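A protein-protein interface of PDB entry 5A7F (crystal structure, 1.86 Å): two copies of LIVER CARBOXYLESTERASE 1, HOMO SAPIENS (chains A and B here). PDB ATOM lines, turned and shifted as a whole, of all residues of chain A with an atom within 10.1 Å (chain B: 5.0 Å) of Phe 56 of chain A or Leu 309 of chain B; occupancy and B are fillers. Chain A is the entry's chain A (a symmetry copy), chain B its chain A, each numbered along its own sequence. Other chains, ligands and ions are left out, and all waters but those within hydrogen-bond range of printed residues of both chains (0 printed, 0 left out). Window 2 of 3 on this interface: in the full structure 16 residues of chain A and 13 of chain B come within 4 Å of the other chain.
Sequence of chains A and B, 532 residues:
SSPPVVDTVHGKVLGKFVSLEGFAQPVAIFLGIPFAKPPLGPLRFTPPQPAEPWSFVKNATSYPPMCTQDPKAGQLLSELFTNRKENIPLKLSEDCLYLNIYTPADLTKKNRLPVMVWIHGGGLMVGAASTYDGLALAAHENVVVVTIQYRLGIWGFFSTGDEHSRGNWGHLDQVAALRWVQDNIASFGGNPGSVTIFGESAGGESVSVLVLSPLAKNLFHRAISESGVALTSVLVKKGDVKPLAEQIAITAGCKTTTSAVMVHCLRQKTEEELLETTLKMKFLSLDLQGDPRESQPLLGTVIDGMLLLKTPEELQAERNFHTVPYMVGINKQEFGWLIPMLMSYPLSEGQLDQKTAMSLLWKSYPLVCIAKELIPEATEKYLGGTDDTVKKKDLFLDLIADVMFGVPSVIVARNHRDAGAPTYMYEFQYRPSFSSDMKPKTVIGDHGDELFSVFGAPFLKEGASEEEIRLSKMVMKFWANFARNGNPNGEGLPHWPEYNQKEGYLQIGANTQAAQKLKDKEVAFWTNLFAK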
ATOM      1  N   VAL A   5      25.760 -30.531 -31.446  1.00  0.00           N
ATOM      2  CA  VAL A   5      25.774 -29.628 -30.287  1.00  0.00           C
ATOM      3  C   VAL A   5      27.165 -29.679 -29.653  1.00  0.00           C
ATOM      4  O   VAL A   5      27.641 -30.756 -29.320  1.00  0.00           O
ATOM      5  CB  VAL A   5      24.699 -30.019 -29.246  1.00  0.00           C
ATOM      6  CG1 VAL A   5      24.768 -29.110 -28.015  1.00  0.00           C
ATOM      7  CG2 VAL A   5      23.295 -29.938 -29.849  1.00  0.00           C
ATOM      8  N   VAL A   6      27.814 -28.530 -29.505  1.00  0.00           N
ATOM      9  CA  VAL A   6      29.148 -28.453 -28.890  1.00  0.00           C
ATOM     10  C   VAL A   6      29.257 -27.341 -27.832  1.00  0.00           C
ATOM     11  O   VAL A   6      28.458 -26.382 -27.794  1.00  0.00           O
ATOM     12  CB  VAL A   6      30.272 -28.256 -29.950  1.00  0.00           C
ATOM     13  CG1 VAL A   6      30.228 -29.358 -30.994  1.00  0.00           C
ATOM     14  CG2 VAL A   6      30.157 -26.914 -30.626  1.00  0.00           C
ATOM     15  N   ASP A   7      30.254 -27.514 -26.979  1.00  0.00           N
ATOM     16  CA  ASP A   7      30.559 -26.605 -25.883  1.00  0.00           C
ATOM     17  C   ASP A   7      31.461 -25.492 -26.297  1.00  0.00           C
ATOM     18  O   ASP A   7      32.513 -25.739 -26.891  1.00  0.00           O
ATOM     19  CB  ASP A   7      31.323 -27.344 -24.787  1.00  0.00           C
ATOM     20  CG  ASP A   7      30.475 -28.274 -24.035  1.00  0.00           C
ATOM     21  OD1 ASP A   7      29.295 -27.948 -23.789  1.00  0.00           O
ATOM     22  OD2 ASP A   7      30.997 -29.322 -23.637  1.00  0.00           O
ATOM     23  N   THR A   8      31.050 -24.274 -25.993  1.00  0.00           N
ATOM     24  CA  THR A   8      31.911 -23.107 -26.050  1.00  0.00           C
ATOM     25  C   THR A   8      32.145 -22.646 -24.602  1.00  0.00           C
ATOM     26  O   THR A   8      31.451 -23.091 -23.650  1.00  0.00           O
ATOM     27  CB  THR A   8      31.314 -21.955 -26.917  1.00  0.00           C
ATOM     28  OG1 THR A   8      30.364 -21.182 -26.177  1.00  0.00           O
ATOM     29  CG2 THR A   8      30.656 -22.486 -28.198  1.00  0.00           C
ATOM     30  N   VAL A   9      33.097 -21.728 -24.444  1.00  0.00           N
ATOM     31  CA  VAL A   9      33.386 -21.124 -23.129  1.00  0.00           C
ATOM     32  C   VAL A   9      32.149 -20.422 -22.560  1.00  0.00           C
ATOM     33  O   VAL A   9      32.000 -20.333 -21.366  1.00  0.00           O
ATOM     34  CB  VAL A   9      34.585 -20.132 -23.194  1.00  0.00           C
ATOM     35  CG1 VAL A   9      34.892 -19.586 -21.815  1.00  0.00           C
ATOM     36  CG2 VAL A   9      35.840 -20.835 -23.695  1.00  0.00           C
ATOM     37  N   HIS A  10      31.242 -19.951 -23.421  1.00  0.00           N
ATOM     38  CA  HIS A  10      30.067 -19.221 -22.966  1.00  0.00           C
ATOM     39  C   HIS A  10      28.779 -20.064 -22.902  1.00  0.00           C
ATOM     40  O   HIS A  10      27.728 -19.576 -22.467  1.00  0.00           O
ATOM     41  CB  HIS A  10      29.878 -17.998 -23.852  1.00  0.00           C
ATOM     42  CG  HIS A  10      31.068 -17.093 -23.854  1.00  0.00           C
ATOM     43  ND1 HIS A  10      31.561 -16.519 -22.701  1.00  0.00           N
ATOM     44  CD2 HIS A  10      31.886 -16.690 -24.850  1.00  0.00           C
ATOM     45  CE1 HIS A  10      32.624 -15.793 -22.989  1.00  0.00           C
ATOM     46  NE2 HIS A  10      32.836 -15.874 -24.288  1.00  0.00           N
ATOM     47  N   GLY A  11      28.888 -21.335 -23.282  1.00  0.00           N
ATOM     48  CA  GLY A  11      27.798 -22.287 -23.218  1.00  0.00           C
ATOM     49  C   GLY A  11      27.661 -23.097 -24.501  1.00  0.00           C
ATOM     50  O   GLY A  11      28.443 -22.943 -25.462  1.00  0.00           O
ATOM     51  N   LYS A  12      26.645 -23.939 -24.531  1.00  0.00           N
ATOM     52  CA  LYS A  12      26.413 -24.849 -25.659  1.00  0.00           C
ATOM     53  C   LYS A  12      25.764 -24.179 -26.851  1.00  0.00           C
ATOM     54  O   LYS A  12      24.925 -23.277 -26.691  1.00  0.00           O
ATOM     55  CB  LYS A  12      25.541 -26.025 -25.225  1.00  0.00           C
ATOM     56  CG  LYS A  12      26.183 -26.806 -24.103  1.00  0.00           C
ATOM     57  CD  LYS A  12      25.411 -28.071 -23.780  1.00  0.00           C
ATOM     58  CE  LYS A  12      25.877 -28.648 -22.453  1.00  0.00           C
ATOM     59  NZ  LYS A  12      27.217 -29.272 -22.604  1.00  0.00           N
ATOM     60  N   VAL A  13      26.144 -24.651 -28.050  1.00  0.00           N
ATOM     61  CA  VAL A  13      25.538 -24.182 -29.300  1.00  0.00           C
ATOM     62  C   VAL A  13      25.126 -25.386 -30.158  1.00  0.00           C
ATOM     63  O   VAL A  13      25.825 -26.421 -30.235  1.00  0.00           O
ATOM     64  CB  VAL A  13      26.462 -23.238 -30.128  1.00  0.00           C
ATOM     65  CG1 VAL A  13      26.785 -21.993 -29.329  1.00  0.00           C
ATOM     66  CG2 VAL A  13      27.756 -23.937 -30.528  1.00  0.00           C
ATOM     67  N   LEU A  14      24.002 -25.188 -30.827  1.00  0.00           N
ATOM     68  CA  LEU A  14      23.381 -26.181 -31.683  1.00  0.00           C
ATOM     69  C   LEU A  14      23.539 -25.678 -33.110  1.00  0.00           C
ATOM     70  O   LEU A  14      23.224 -24.513 -33.391  1.00  0.00           O
ATOM     71  CB  LEU A  14      21.919 -26.284 -31.311  1.00  0.00           C
ATOM     72  CG  LEU A  14      20.871 -27.096 -32.060  1.00  0.00           C
ATOM     73  CD1 LEU A  14      20.173 -26.346 -33.183  1.00  0.00           C
ATOM     74  CD2 LEU A  14      21.408 -28.379 -32.578  1.00  0.00           C
ATOM     75  N   PRO A  53      27.675 -15.199 -20.762  1.00  0.00           N
ATOM     76  CA  PRO A  53      27.396 -16.640 -20.932  1.00  0.00           C
ATOM     77  C   PRO A  53      25.883 -16.932 -20.933  1.00  0.00           C
ATOM     78  O   PRO A  53      25.113 -16.197 -20.328  1.00  0.00           O
ATOM     79  CB  PRO A  53      28.062 -17.282 -19.720  1.00  0.00           C
ATOM     80  CG  PRO A  53      28.151 -16.184 -18.692  1.00  0.00           C
ATOM     81  CD  PRO A  53      28.304 -14.899 -19.458  1.00  0.00           C
ATOM     82  N   TRP A  54      25.473 -18.025 -21.566  1.00  0.00           N
ATOM     83  CA  TRP A  54      24.071 -18.403 -21.632  1.00  0.00           C
ATOM     84  C   TRP A  54      23.835 -19.769 -21.034  1.00  0.00           C
ATOM     85  O   TRP A  54      24.734 -20.612 -20.972  1.00  0.00           O
ATOM     86  CB  TRP A  54      23.538 -18.319 -23.076  1.00  0.00           C
ATOM     87  CG  TRP A  54      24.332 -19.123 -24.034  1.00  0.00           C
ATOM     88  CD1 TRP A  54      24.147 -20.422 -24.346  1.00  0.00           C
ATOM     89  CD2 TRP A  54      25.463 -18.680 -24.782  1.00  0.00           C
ATOM     90  NE1 TRP A  54      25.070 -20.828 -25.269  1.00  0.00           N
ATOM     91  CE2 TRP A  54      25.896 -19.778 -25.563  1.00  0.00           C
ATOM     92  CE3 TRP A  54      26.114 -17.447 -24.924  1.00  0.00           C
ATOM     93  CZ2 TRP A  54      26.984 -19.700 -26.426  1.00  0.00           C
ATOM     94  CZ3 TRP A  54      27.190 -17.362 -25.790  1.00  0.00           C
ATOM     95  CH2 TRP A  54      27.618 -18.488 -26.535  1.00  0.00           C
ATOM     96  N   SER A  55      22.612 -19.972 -20.558  1.00  0.00           N
ATOM     97  CA  SER A  55      22.171 -21.259 -20.048  1.00  0.00           C
ATOM     98  C   SER A  55      21.629 -22.074 -21.230  1.00  0.00           C
ATOM     99  O   SER A  55      21.310 -21.519 -22.286  1.00  0.00           O
ATOM    100  CB  SER A  55      21.080 -21.061 -18.977  1.00  0.00           C
ATOM    101  OG  SER A  55      21.384 -19.937 -18.173  1.00  0.00           O
ATOM    102  N   PHE A  56      21.527 -23.370 -21.050  1.00  0.00           N
ATOM    103  CA  PHE A  56      20.863 -24.228 -22.041  1.00  0.00           C
ATOM    104  C   PHE A  56      21.621 -24.173 -23.374  1.00  0.00           C
ATOM    105  O   PHE A  56      22.846 -23.973 -23.378  1.00  0.00           O
ATOM    106  CB  PHE A  56      19.352 -23.878 -22.193  1.00  0.00           C
ATOM    107  CG  PHE A  56      18.613 -23.711 -20.886  1.00  0.00           C
ATOM    108  CD1 PHE A  56      18.603 -24.724 -19.930  1.00  0.00           C
ATOM    109  CD2 PHE A  56      17.893 -22.557 -20.620  1.00  0.00           C
ATOM    110  CE1 PHE A  56      17.928 -24.556 -18.723  1.00  0.00           C
ATOM    111  CE2 PHE A  56      17.212 -22.388 -19.415  1.00  0.00           C
ATOM    112  CZ  PHE A  56      17.235 -23.389 -18.474  1.00  0.00           C
ATOM    113  N   VAL A  57      20.950 -24.402 -24.494  1.00  0.00           N
ATOM    114  CA  VAL A  57      21.645 -24.580 -25.777  1.00  0.00           C
ATOM    115  C   VAL A  57      21.230 -23.447 -26.711  1.00  0.00           C
ATOM    116  O   VAL A  57      20.022 -23.208 -26.906  1.00  0.00           O
ATOM    117  CB  VAL A  57      21.325 -25.931 -26.438  1.00  0.00           C
ATOM    118  CG1 VAL A  57      22.121 -26.081 -27.723  1.00  0.00           C
ATOM    119  CG2 VAL A  57      21.618 -27.093 -25.484  1.00  0.00           C
ATOM    120  N   LYS A  58      22.216 -22.693 -27.198  1.00  0.00           N
ATOM    121  CA  LYS A  58      21.941 -21.607 -28.146  1.00  0.00           C
ATOM    122  C   LYS A  58      21.741 -22.188 -29.551  1.00  0.00           C
ATOM    123  O   LYS A  58      22.598 -22.890 -30.096  1.00  0.00           O
ATOM    124  CB  LYS A  58      23.061 -20.550 -28.133  1.00  0.00           C
ATOM    125  CG  LYS A  58      22.781 -19.386 -29.084  1.00  0.00           C
ATOM    126  CD  LYS A  58      23.894 -18.343 -29.045  1.00  0.00           C
ATOM    127  CE  LYS A  58      23.936 -17.564 -27.750  1.00  0.00           C
ATOM    128  NZ  LYS A  58      22.708 -16.791 -27.500  1.00  0.00           N
ATOM    129  N   ASN A  59      20.611 -21.852 -30.148  1.00  0.00           N
ATOM    130  CA  ASN A  59      20.299 -22.285 -31.492  1.00  0.00           C
ATOM    131  C   ASN A  59      21.035 -21.407 -32.531  1.00  0.00           C
ATOM    132  O   ASN A  59      20.654 -20.290 -32.788  1.00  0.00           O
ATOM    133  CB  ASN A  59      18.781 -22.270 -31.686  1.00  0.00           C
ATOM    134  CG  ASN A  59      18.360 -22.886 -33.000  1.00  0.00           C
ATOM    135  OD1 ASN A  59      19.195 -23.131 -33.900  1.00  0.00           O
ATOM    136  ND2 ASN A  59      17.052 -23.138 -33.137  1.00  0.00           N
ATOM    137  N   ALA A  60      22.130 -21.923 -33.076  1.00  0.00           N
ATOM    138  CA  ALA A  60      22.977 -21.190 -34.034  1.00  0.00           C
ATOM    139  C   ALA A  60      22.698 -21.634 -35.474  1.00  0.00           C
ATOM    140  O   ALA A  60      23.562 -22.234 -36.150  1.00  0.00           O
ATOM    141  CB  ALA A  60      24.436 -21.415 -33.677  1.00  0.00           C
ATOM    142  N   PRO B 214      17.516 -22.933  -6.323  1.00  0.00           N
ATOM    143  CA  PRO B 214      18.791 -22.999  -5.590  1.00  0.00           C
ATOM    144  C   PRO B 214      19.304 -21.608  -5.162  1.00  0.00           C
ATOM    145  O   PRO B 214      20.083 -21.524  -4.229  1.00  0.00           O
ATOM    146  CB  PRO B 214      19.765 -23.642  -6.597  1.00  0.00           C
ATOM    147  CG  PRO B 214      19.232 -23.228  -7.934  1.00  0.00           C
ATOM    148  CD  PRO B 214      17.713 -23.168  -7.768  1.00  0.00           C
ATOM    149  N   ILE B 303      11.657 -20.079 -17.149  1.00  0.00           N
ATOM    150  CA  ILE B 303      12.704 -21.034 -16.739  1.00  0.00           C
ATOM    151  C   ILE B 303      13.993 -20.409 -17.267  1.00  0.00           C
ATOM    152  O   ILE B 303      14.300 -20.528 -18.418  1.00  0.00           O
ATOM    153  CB  ILE B 303      12.499 -22.454 -17.339  1.00  0.00           C
ATOM    154  CG1 ILE B 303      11.084 -22.992 -17.049  1.00  0.00           C
ATOM    155  CG2 ILE B 303      13.599 -23.410 -16.865  1.00  0.00           C
ATOM    156  CD1 ILE B 303      10.621 -22.847 -15.631  1.00  0.00           C
ATOM    157  N   ASP B 304      14.700 -19.679 -16.428  1.00  0.00           N
ATOM    158  CA  ASP B 304      15.784 -18.778 -16.865  1.00  0.00           C
ATOM    159  C   ASP B 304      17.179 -19.403 -16.722  1.00  0.00           C
ATOM    160  O   ASP B 304      18.162 -18.854 -17.212  1.00  0.00           O
ATOM    161  CB  ASP B 304      15.738 -17.500 -16.038  1.00  0.00           C
ATOM    162  CG  ASP B 304      15.978 -17.745 -14.527  1.00  0.00           C
ATOM    163  OD1 ASP B 304      15.637 -18.826 -13.995  1.00  0.00           O
ATOM    164  OD2 ASP B 304      16.487 -16.858 -13.839  1.00  0.00           O
ATOM    165  N   GLY B 305      17.279 -20.530 -16.032  1.00  0.00           N
ATOM    166  CA  GLY B 305      18.569 -21.180 -15.811  1.00  0.00           C
ATOM    167  C   GLY B 305      19.390 -20.624 -14.653  1.00  0.00           C
ATOM    168  O   GLY B 305      20.486 -21.066 -14.431  1.00  0.00           O
ATOM    169  N   MET B 306      18.874 -19.636 -13.932  1.00  0.00           N
ATOM    170  CA  MET B 306      19.562 -19.038 -12.769  1.00  0.00           C
ATOM    171  C   MET B 306      18.665 -19.221 -11.533  1.00  0.00           C
ATOM    172  O   MET B 306      19.022 -19.887 -10.561  1.00  0.00           O
ATOM    173  CB  MET B 306      19.803 -17.542 -13.012  1.00  0.00           C
ATOM    174  CG  MET B 306      20.812 -17.184 -14.089  1.00  0.00           C
ATOM    175  SD  MET B 306      22.510 -17.696 -13.740  1.00  0.00           S
ATOM    176  CE  MET B 306      22.599 -17.245 -12.010  1.00  0.00           C
ATOM    177  N   LEU B 307      17.473 -18.623 -11.579  1.00  0.00           N
ATOM    178  CA  LEU B 307      16.480 -18.851 -10.542  1.00  0.00           C
ATOM    179  C   LEU B 307      15.820 -20.238 -10.632  1.00  0.00           C
ATOM    180  O   LEU B 307      15.711 -20.935  -9.638  1.00  0.00           O
ATOM    181  CB  LEU B 307      15.391 -17.789 -10.609  1.00  0.00           C
ATOM    182  CG  LEU B 307      14.327 -17.945  -9.528  1.00  0.00           C
ATOM    183  CD1 LEU B 307      14.702 -17.203  -8.269  1.00  0.00           C
ATOM    184  CD2 LEU B 307      13.001 -17.468 -10.057  1.00  0.00           C
ATOM    185  N   LEU B 308      15.366 -20.618 -11.818  1.00  0.00           N
ATOM    186  CA  LEU B 308      14.782 -21.936 -12.060  1.00  0.00           C
ATOM    187  C   LEU B 308      15.540 -22.618 -13.154  1.00  0.00           C
ATOM    188  O   LEU B 308      15.606 -22.081 -14.249  1.00  0.00           O
ATOM    189  CB  LEU B 308      13.313 -21.792 -12.529  1.00  0.00           C
ATOM    190  CG  LEU B 308      12.271 -21.417 -11.505  1.00  0.00           C
ATOM    191  CD1 LEU B 308      10.884 -21.259 -12.149  1.00  0.00           C
ATOM    192  CD2 LEU B 308      12.219 -22.469 -10.413  1.00  0.00           C
ATOM    193  N   LEU B 309      16.068 -23.801 -12.858  1.00  0.00           N
ATOM    194  CA  LEU B 309      16.869 -24.581 -13.771  1.00  0.00           C
ATOM    195  C   LEU B 309      16.034 -25.479 -14.699  1.00  0.00           C
ATOM    196  O   LEU B 309      16.511 -25.865 -15.760  1.00  0.00           O
ATOM    197  CB  LEU B 309      17.873 -25.437 -12.998  1.00  0.00           C
ATOM    198  CG  LEU B 309      18.771 -24.716 -11.982  1.00  0.00           C
ATOM    199  CD1 LEU B 309      19.951 -25.584 -11.578  1.00  0.00           C
ATOM    200  CD2 LEU B 309      19.284 -23.397 -12.522  1.00  0.00           C
ATOM    201  N   LYS B 310      14.816 -25.821 -14.284  1.00  0.00           N
ATOM    202  CA  LYS B 310      13.880 -26.647 -15.072  1.00  0.00           C
ATOM    203  C   LYS B 310      12.462 -26.232 -14.749  1.00  0.00           C
ATOM    204  O   LYS B 310      12.253 -25.396 -13.875  1.00  0.00           O
ATOM    205  CB  LYS B 310      14.005 -28.127 -14.698  1.00  0.00           C
ATOM    206  CG  LYS B 310      15.393 -28.697 -14.843  1.00  0.00           C
ATOM    207  CD  LYS B 310      15.471 -30.129 -14.315  1.00  0.00           C
ATOM    208  CE  LYS B 310      16.937 -30.529 -14.234  1.00  0.00           C
ATOM    209  NZ  LYS B 310      17.146 -31.991 -14.369  1.00  0.00           N
ATOM    210  N   THR B 311      11.481 -26.862 -15.393  1.00  0.00           N
ATOM    211  CA  THR B 311      10.091 -26.547 -15.089  1.00  0.00           C
ATOM    212  C   THR B 311       9.750 -27.027 -13.675  1.00  0.00           C
ATOM    213  O   THR B 311      10.341 -27.962 -13.173  1.00  0.00           O
ATOM    214  CB  THR B 311       9.092 -27.146 -16.097  1.00  0.00           C
ATOM    215  OG1 THR B 311       9.072 -28.568 -15.972  1.00  0.00           O
ATOM    216  CG2 THR B 311       9.476 -26.796 -17.498  1.00  0.00           C
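The backbone NH (N) of Met 306 of chain B sits close to the side-chain carboxylate (OD1) of Asp 304 of chain B.
The backbone NH (N) of Leu 307 of chain B lies within hydrogen-bond range of the side-chain carboxylate (OD2) of Asp 304 of chain B.
The side-chain carboxylate (OD1) of Asp 304 of chain B is in hydrogen-bond range of the backbone NH (N) of Leu 308 of chain B (2.8 Å).
Among the printed residues, merely in contact across the chains: Ser 55 of chain A with Asp 304 of chain B, Ser 55 of chain A with Gly 305 of chain B, Phe 56 of chain A with Ile 303 of chain B, Phe 56 of chain A with Gly 305 of chain B and Phe 56 of chain A with Leu 309 of chain B.
Of the printed residues of chain B, Ser 55 of chain A touches Asp 304 and Gly 305.
Of chain B, only Ile 303 (3.6 Å), Gly 305 (3.7 Å) and Leu 309 (3.5 Å) come within 4 Å of Phe 56 of chain A.
Printed residues of chain A within 4 Å of Ile 303 of chain B: Phe 56.
No residue of chain A comes within 4 Å of Leu 308 of chain B.
Leu 309 of chain B touches just one residue of chain A: Phe 56 (3.5 Å).
The nearest residue of chain B that does not touch Phe 56 of chain A is Asp 304 of chain B (4.02 Å).
The nearest printed residue of chain B that does not touch Ser 55 of chain A is Met 306 of chain B (4.9 Å).
Of the 10 printed residues of chain B, 4 touch a printed residue of chain A.
Along chain B the printed residues that touch a printed residue of chain A span positions 303 to 309.
Hydrophobic or aromatic side chains of chain A that line the printed part of chain B: Phe 56.
Among the printed residues, 5 pairs touch across the chains.
Among the printed residues, no Asp or Glu carboxylate lies within 4 Å of a Lys or Arg side-chain nitrogen of the other chain.
No position is printed for both chains.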
